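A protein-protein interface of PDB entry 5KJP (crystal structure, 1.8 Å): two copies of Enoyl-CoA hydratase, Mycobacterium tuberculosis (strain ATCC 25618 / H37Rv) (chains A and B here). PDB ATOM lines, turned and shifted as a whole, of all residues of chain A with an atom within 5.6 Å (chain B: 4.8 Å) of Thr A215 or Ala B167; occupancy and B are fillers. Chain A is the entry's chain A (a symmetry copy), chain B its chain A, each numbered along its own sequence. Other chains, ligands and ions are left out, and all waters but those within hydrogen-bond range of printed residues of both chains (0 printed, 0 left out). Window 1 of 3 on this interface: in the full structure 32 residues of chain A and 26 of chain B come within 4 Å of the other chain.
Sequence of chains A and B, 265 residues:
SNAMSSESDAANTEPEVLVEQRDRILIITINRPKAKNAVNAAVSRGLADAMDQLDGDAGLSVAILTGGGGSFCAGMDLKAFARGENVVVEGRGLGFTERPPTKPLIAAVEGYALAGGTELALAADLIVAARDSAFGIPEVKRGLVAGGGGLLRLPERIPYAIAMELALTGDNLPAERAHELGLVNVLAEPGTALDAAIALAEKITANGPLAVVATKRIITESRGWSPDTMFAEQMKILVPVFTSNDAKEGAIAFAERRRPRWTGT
The side-chain hydroxyl (OG1) of Thr A215 lies within hydrogen-bond range of the backbone carbonyl oxygen (O) of Ala A211, 2.8 Å away.
Ala A211 touches Val B145 (O to CG2, 3.7 Å). Val A212 touches Leu B168 (O to CD2, 3.5 Å). Thr A215 touches Val B140 (OG1 to CG1, 3.4 Å). CD2 of Leu B151 touches CG2 of Thr A215, at 3.7 Å. Ala B167 touches Thr A215. Thr A215 touches Leu B168. CG1 of Val B145 touches CD1 of Ile A218, at 3.9 Å. Ile A218 touches Leu B151. Leu B151 touches Ile A219. Ala B167 touches Ile A219 (CB to CD1, 3.8 Å).
Of chain B, only Val B140, Val B145, Leu B151, Ala B167 and Leu B168 come within 4 Å of Thr A215. Of chain A, only Thr A215 and Ile A219 come within 4 Å of Ala B167. Of the printed residues of chain A, Leu B151 touches Thr A215 (3.7 Å), Ile A218 (3.8 Å) and Ile A219 (3.9 Å). Printed residues of chain B within 4 Å of Val A212: Leu B168 (3.5 Å). Leu A210 touches none of the printed residues of chain B. Val A213 touches none of the printed residues of chain B.
No position is printed for both chains. Of the 14 pairs that touch across the chains among the printed residues, none has its exchanged pair printed and touching as well.
Along chain B the printed residues that touch a printed residue of chain A span positions 140 to 168. Of the 11 printed residues of chain A, 5 touch a printed residue of chain B. Among the printed residues, no Asp or Glu carboxylate lies within 4 Å of a Lys or Arg side-chain nitrogen of the other chain.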
ATOM      1  N   LEU A 210     -21.556  -8.723  -2.791  1.00  0.00           N
ATOM      2  CA  LEU A 210     -21.270  -7.323  -2.469  1.00  0.00           C
ATOM      3  C   LEU A 210     -20.654  -6.600  -3.662  1.00  0.00           C
ATOM      4  O   LEU A 210     -20.950  -5.434  -3.915  1.00  0.00           O
ATOM      5  CB  LEU A 210     -20.336  -7.220  -1.261  1.00  0.00           C
ATOM      6  CG  LEU A 210     -20.860  -7.851   0.029  1.00  0.00           C
ATOM      7  CD1 LEU A 210     -19.772  -7.857   1.100  1.00  0.00           C
ATOM      8  CD2 LEU A 210     -22.115  -7.120   0.511  1.00  0.00           C
ATOM      9  N   ALA A 211     -19.789  -7.300  -4.387  1.00  0.00           N
ATOM     10  CA  ALA A 211     -19.109  -6.711  -5.535  1.00  0.00           C
ATOM     11  C   ALA A 211     -20.092  -6.478  -6.679  1.00  0.00           C
ATOM     12  O   ALA A 211     -20.039  -5.452  -7.351  1.00  0.00           O
ATOM     13  CB  ALA A 211     -17.951  -7.601  -5.985  1.00  0.00           C
ATOM     14  N   VAL A 212     -21.001  -7.427  -6.882  1.00  0.00           N
ATOM     15  CA  VAL A 212     -22.026  -7.298  -7.914  1.00  0.00           C
ATOM     16  C   VAL A 212     -22.942  -6.102  -7.633  1.00  0.00           C
ATOM     17  O   VAL A 212     -23.206  -5.284  -8.522  1.00  0.00           O
ATOM     18  CB  VAL A 212     -22.860  -8.599  -8.023  1.00  0.00           C
ATOM     19  CG1 VAL A 212     -24.162  -8.354  -8.772  1.00  0.00           C
ATOM     20  CG2 VAL A 212     -22.037  -9.706  -8.697  1.00  0.00           C
ATOM     21  N   VAL A 213     -23.396  -5.980  -6.390  1.00  0.00           N
ATOM     22  CA  VAL A 213     -24.309  -4.899  -6.038  1.00  0.00           C
ATOM     23  C   VAL A 213     -23.587  -3.558  -6.125  1.00  0.00           C
ATOM     24  O   VAL A 213     -24.147  -2.578  -6.624  1.00  0.00           O
ATOM     25  CB  VAL A 213     -24.915  -5.098  -4.633  1.00  0.00           C
ATOM     26  CG1 VAL A 213     -25.428  -3.780  -4.059  1.00  0.00           C
ATOM     27  CG2 VAL A 213     -26.031  -6.142  -4.687  1.00  0.00           C
ATOM     28  N   ALA A 214     -22.335  -3.520  -5.669  1.00  0.00           N
ATOM     29  CA  ALA A 214     -21.542  -2.293  -5.738  1.00  0.00           C
ATOM     30  C   ALA A 214     -21.276  -1.890  -7.178  1.00  0.00           C
ATOM     31  O   ALA A 214     -21.254  -0.704  -7.505  1.00  0.00           O
ATOM     32  CB  ALA A 214     -20.224  -2.461  -4.994  1.00  0.00           C
ATOM     33  N   THR A 215     -21.068  -2.882  -8.035  1.00  0.00           N
ATOM     34  CA  THR A 215     -20.792  -2.623  -9.442  1.00  0.00           C
ATOM     35  C   THR A 215     -22.011  -1.987 -10.105  1.00  0.00           C
ATOM     36  O   THR A 215     -21.894  -0.991 -10.827  1.00  0.00           O
ATOM     37  CB  THR A 215     -20.393  -3.915 -10.176  1.00  0.00           C
ATOM     38  OG1 THR A 215     -19.107  -4.343  -9.703  1.00  0.00           O
ATOM     39  CG2 THR A 215     -20.306  -3.676 -11.677  1.00  0.00           C
ATOM     40  N   LYS A 216     -23.185  -2.549  -9.834  1.00  0.00           N
ATOM     41  CA  LYS A 216     -24.418  -1.986 -10.365  1.00  0.00           C
ATOM     42  C   LYS A 216     -24.631  -0.577  -9.829  1.00  0.00           C
ATOM     43  O   LYS A 216     -25.016   0.332 -10.568  1.00  0.00           O
ATOM     44  CB  LYS A 216     -25.620  -2.873 -10.025  1.00  0.00           C
ATOM     45  CG  LYS A 216     -26.951  -2.199 -10.306  1.00  0.00           C
ATOM     46  CD  LYS A 216     -28.140  -3.140 -10.145  1.00  0.00           C
ATOM     47  CE  LYS A 216     -29.437  -2.343 -10.112  1.00  0.00           C
ATOM     48  NZ  LYS A 216     -30.651  -3.218 -10.159  1.00  0.00           N
ATOM     49  N   ARG A 217     -24.375  -0.402  -8.538  1.00  0.00           N
ATOM     50  CA  ARG A 217     -24.537   0.893  -7.906  1.00  0.00           C
ATOM     51  C   ARG A 217     -23.664   1.962  -8.566  1.00  0.00           C
ATOM     52  O   ARG A 217     -24.116   3.080  -8.810  1.00  0.00           O
ATOM     53  CB  ARG A 217     -24.213   0.799  -6.416  1.00  0.00           C
ATOM     54  CG  ARG A 217     -24.499   2.078  -5.681  1.00  0.00           C
ATOM     55  CD  ARG A 217     -24.371   1.917  -4.178  1.00  0.00           C
ATOM     56  NE  ARG A 217     -24.429   3.218  -3.522  1.00  0.00           N
ATOM     57  CZ  ARG A 217     -24.075   3.436  -2.263  1.00  0.00           C
ATOM     58  NH1 ARG A 217     -23.639   2.432  -1.511  1.00  0.00           N
ATOM     59  NH2 ARG A 217     -24.158   4.660  -1.759  1.00  0.00           N
ATOM     60  N   ILE A 218     -22.414   1.623  -8.860  1.00  0.00           N
ATOM     61  CA  ILE A 218     -21.511   2.605  -9.450  1.00  0.00           C
ATOM     62  C   ILE A 218     -21.969   2.946 -10.869  1.00  0.00           C
ATOM     63  O   ILE A 218     -22.031   4.116 -11.234  1.00  0.00           O
ATOM     64  CB  ILE A 218     -20.048   2.103  -9.451  1.00  0.00           C
ATOM     65  CG1 ILE A 218     -19.504   2.090  -8.018  1.00  0.00           C
ATOM     66  CG2 ILE A 218     -19.162   2.987 -10.333  1.00  0.00           C
ATOM     67  CD1 ILE A 218     -18.326   1.159  -7.819  1.00  0.00           C
ATOM     68  N   ILE A 219     -22.326   1.939 -11.659  1.00  0.00           N
ATOM     69  CA  ILE A 219     -22.777   2.213 -13.026  1.00  0.00           C
ATOM     70  C   ILE A 219     -24.054   3.073 -13.043  1.00  0.00           C
ATOM     71  O   ILE A 219     -24.145   4.040 -13.805  1.00  0.00           O
ATOM     72  CB  ILE A 219     -23.004   0.914 -13.815  1.00  0.00           C
ATOM     73  CG1 ILE A 219     -21.653   0.227 -14.076  1.00  0.00           C
ATOM     74  CG2 ILE A 219     -23.726   1.204 -15.134  1.00  0.00           C
ATOM     75  CD1 ILE A 219     -21.759  -1.125 -14.764  1.00  0.00           C
ATOM     76  N   THR A 220     -25.016   2.751 -12.180  1.00  0.00           N
ATOM     77  CA  THR A 220     -26.266   3.516 -12.136  1.00  0.00           C
ATOM     78  C   THR A 220     -26.065   4.925 -11.563  1.00  0.00           C
ATOM     79  O   THR A 220     -26.560   5.897 -12.121  1.00  0.00           O
ATOM     80  CB  THR A 220     -27.373   2.788 -11.313  1.00  0.00           C
ATOM     81  OG1 THR A 220     -26.980   2.685  -9.939  1.00  0.00           O
ATOM     82  CG2 THR A 220     -27.648   1.388 -11.868  1.00  0.00           C
ATOM     83  N   ILE B 137     -13.786  -7.192 -17.782  1.00  0.00           N
ATOM     84  CA  ILE B 137     -13.575  -6.713 -16.423  1.00  0.00           C
ATOM     85  C   ILE B 137     -14.117  -7.769 -15.453  1.00  0.00           C
ATOM     86  O   ILE B 137     -15.249  -7.675 -14.966  1.00  0.00           O
ATOM     87  CB  ILE B 137     -14.242  -5.338 -16.184  1.00  0.00           C
ATOM     88  CG1 ILE B 137     -15.626  -5.272 -16.846  1.00  0.00           C
ATOM     89  CG2 ILE B 137     -13.357  -4.220 -16.754  1.00  0.00           C
ATOM     90  CD1 ILE B 137     -16.422  -4.009 -16.478  1.00  0.00           C
ATOM     91  N   VAL B 140     -15.481  -8.840 -10.442  1.00  0.00           N
ATOM     92  CA  VAL B 140     -16.523  -9.360  -9.547  1.00  0.00           C
ATOM     93  C   VAL B 140     -16.359 -10.853  -9.269  1.00  0.00           C
ATOM     94  O   VAL B 140     -16.857 -11.356  -8.268  1.00  0.00           O
ATOM     95  CB  VAL B 140     -17.949  -9.120 -10.109  1.00  0.00           C
ATOM     96  CG1 VAL B 140     -18.302  -7.630 -10.077  1.00  0.00           C
ATOM     97  CG2 VAL B 140     -18.086  -9.712 -11.508  1.00  0.00           C
ATOM     98  N   LEU B 144     -14.260  -8.444  -6.123  1.00  0.00           N
ATOM     99  CA  LEU B 144     -13.768  -7.073  -6.228  1.00  0.00           C
ATOM    100  C   LEU B 144     -14.531  -6.285  -7.288  1.00  0.00           C
ATOM    101  O   LEU B 144     -15.430  -6.805  -7.940  1.00  0.00           O
ATOM    102  CB  LEU B 144     -12.271  -7.061  -6.543  1.00  0.00           C
ATOM    103  CG  LEU B 144     -11.390  -7.671  -5.445  1.00  0.00           C
ATOM    104  CD1 LEU B 144      -9.916  -7.590  -5.829  1.00  0.00           C
ATOM    105  CD2 LEU B 144     -11.644  -6.990  -4.100  1.00  0.00           C
ATOM    106  N   VAL B 145     -14.157  -5.024  -7.455  1.00  0.00           N
ATOM    107  CA  VAL B 145     -14.854  -4.129  -8.365  1.00  0.00           C
ATOM    108  C   VAL B 145     -13.826  -3.449  -9.270  1.00  0.00           C
ATOM    109  O   VAL B 145     -12.728  -3.126  -8.819  1.00  0.00           O
ATOM    110  CB  VAL B 145     -15.675  -3.086  -7.572  1.00  0.00           C
ATOM    111  CG1 VAL B 145     -16.301  -2.062  -8.496  1.00  0.00           C
ATOM    112  CG2 VAL B 145     -16.744  -3.783  -6.724  1.00  0.00           C
ATOM    113  N   LEU B 151     -15.839   0.896 -14.733  1.00  0.00           N
ATOM    114  CA  LEU B 151     -17.269   1.094 -14.531  1.00  0.00           C
ATOM    115  C   LEU B 151     -17.702   2.501 -14.923  1.00  0.00           C
ATOM    116  O   LEU B 151     -18.862   2.724 -15.252  1.00  0.00           O
ATOM    117  CB  LEU B 151     -17.643   0.823 -13.082  1.00  0.00           C
ATOM    118  CG  LEU B 151     -17.328  -0.580 -12.572  1.00  0.00           C
ATOM    119  CD1 LEU B 151     -17.987  -0.759 -11.220  1.00  0.00           C
ATOM    120  CD2 LEU B 151     -17.807  -1.630 -13.582  1.00  0.00           C
ATOM    121  N   ALA B 163     -22.517  -3.011 -21.193  1.00  0.00           N
ATOM    122  CA  ALA B 163     -21.519  -2.663 -20.186  1.00  0.00           C
ATOM    123  C   ALA B 163     -21.907  -3.247 -18.820  1.00  0.00           C
ATOM    124  O   ALA B 163     -21.072  -3.828 -18.131  1.00  0.00           O
ATOM    125  CB  ALA B 163     -21.349  -1.152 -20.107  1.00  0.00           C
ATOM    126  N   MET B 164     -23.177  -3.096 -18.448  1.00  0.00           N
ATOM    127  CA  MET B 164     -23.723  -3.712 -17.232  1.00  0.00           C
ATOM    128  C   MET B 164     -23.499  -5.224 -17.227  1.00  0.00           C
ATOM    129  O   MET B 164     -23.022  -5.795 -16.236  1.00  0.00           O
ATOM    130  CB  MET B 164     -25.225  -3.407 -17.101  1.00  0.00           C
ATOM    131  CG  MET B 164     -25.894  -3.964 -15.834  1.00  0.00           C
ATOM    132  SD  MET B 164     -25.290  -3.063 -14.196  1.00  0.00           S
ATOM    133  CE  MET B 164     -26.277  -1.379 -14.422  1.00  0.00           C
ATOM    134  N   GLU B 165     -23.840  -5.874 -18.336  1.00  0.00           N
ATOM    135  CA  GLU B 165     -23.713  -7.325 -18.443  1.00  0.00           C
ATOM    136  C   GLU B 165     -22.270  -7.766 -18.233  1.00  0.00           C
ATOM    137  O   GLU B 165     -21.988  -8.687 -17.453  1.00  0.00           O
ATOM    138  CB  GLU B 165     -24.206  -7.813 -19.805  1.00  0.00           C
ATOM    139  CG  GLU B 165     -23.931  -9.282 -20.060  1.00  0.00           C
ATOM    140  CD  GLU B 165     -24.187  -9.691 -21.505  1.00  0.00           C
ATOM    141  OE1 GLU B 165     -24.761  -8.889 -22.278  1.00  0.00           O
ATOM    142  OE2 GLU B 165     -23.800 -10.821 -21.870  1.00  0.00           O
ATOM    143  N   LEU B 166     -21.351  -7.095 -18.919  1.00  0.00           N
ATOM    144  CA  LEU B 166     -19.938  -7.436 -18.800  1.00  0.00           C
ATOM    145  C   LEU B 166     -19.433  -7.207 -17.378  1.00  0.00           C
ATOM    146  O   LEU B 166     -18.649  -8.001 -16.849  1.00  0.00           O
ATOM    147  CB  LEU B 166     -19.119  -6.624 -19.803  1.00  0.00           C
ATOM    148  CG  LEU B 166     -19.388  -6.994 -21.262  1.00  0.00           C
ATOM    149  CD1 LEU B 166     -18.749  -5.966 -22.199  1.00  0.00           C
ATOM    150  CD2 LEU B 166     -18.880  -8.409 -21.572  1.00  0.00           C
ATOM    151  N   ALA B 167     -19.896  -6.133 -16.752  1.00  0.00           N
ATOM    152  CA  ALA B 167     -19.449  -5.797 -15.407  1.00  0.00           C
ATOM    153  C   ALA B 167     -19.980  -6.786 -14.356  1.00  0.00           C
ATOM    154  O   ALA B 167     -19.272  -7.129 -13.402  1.00  0.00           O
ATOM    155  CB  ALA B 167     -19.865  -4.366 -15.058  1.00  0.00           C
ATOM    156  N   LEU B 168     -21.213  -7.253 -14.530  1.00  0.00           N
ATOM    157  CA  LEU B 168     -21.833  -8.137 -13.538  1.00  0.00           C
ATOM    158  C   LEU B 168     -21.435  -9.600 -13.719  1.00  0.00           C
ATOM    159  O   LEU B 168     -21.407 -10.366 -12.755  1.00  0.00           O
ATOM    160  CB  LEU B 168     -23.360  -8.017 -13.588  1.00  0.00           C
ATOM    161  CG  LEU B 168     -23.944  -6.643 -13.245  1.00  0.00           C
ATOM    162  CD1 LEU B 168     -25.462  -6.705 -13.150  1.00  0.00           C
ATOM    163  CD2 LEU B 168     -23.339  -6.104 -11.955  1.00  0.00           C
ATOM    164  N   THR B 169     -21.154  -9.994 -14.960  1.00  0.00           N
ATOM    165  CA  THR B 169     -20.784 -11.378 -15.244  1.00  0.00           C
ATOM    166  C   THR B 169     -19.279 -11.599 -15.199  1.00  0.00           C
ATOM    167  O   THR B 169     -18.819 -12.684 -14.836  1.00  0.00           O
ATOM    168  CB  THR B 169     -21.273 -11.838 -16.629  1.00  0.00           C
ATOM    169  OG1 THR B 169     -20.639 -11.049 -17.645  1.00  0.00           O
ATOM    170  CG2 THR B 169     -22.806 -11.738 -16.748  1.00  0.00           C
ATOM    171  N   GLY B 170     -18.518 -10.579 -15.594  1.00  0.00           N
ATOM    172  CA  GLY B 170     -17.076 -10.707 -15.751  1.00  0.00           C
ATOM    173  C   GLY B 170     -16.677 -11.455 -17.017  1.00  0.00           C
ATOM    174  O   GLY B 170     -15.530 -11.890 -17.148  1.00  0.00           O
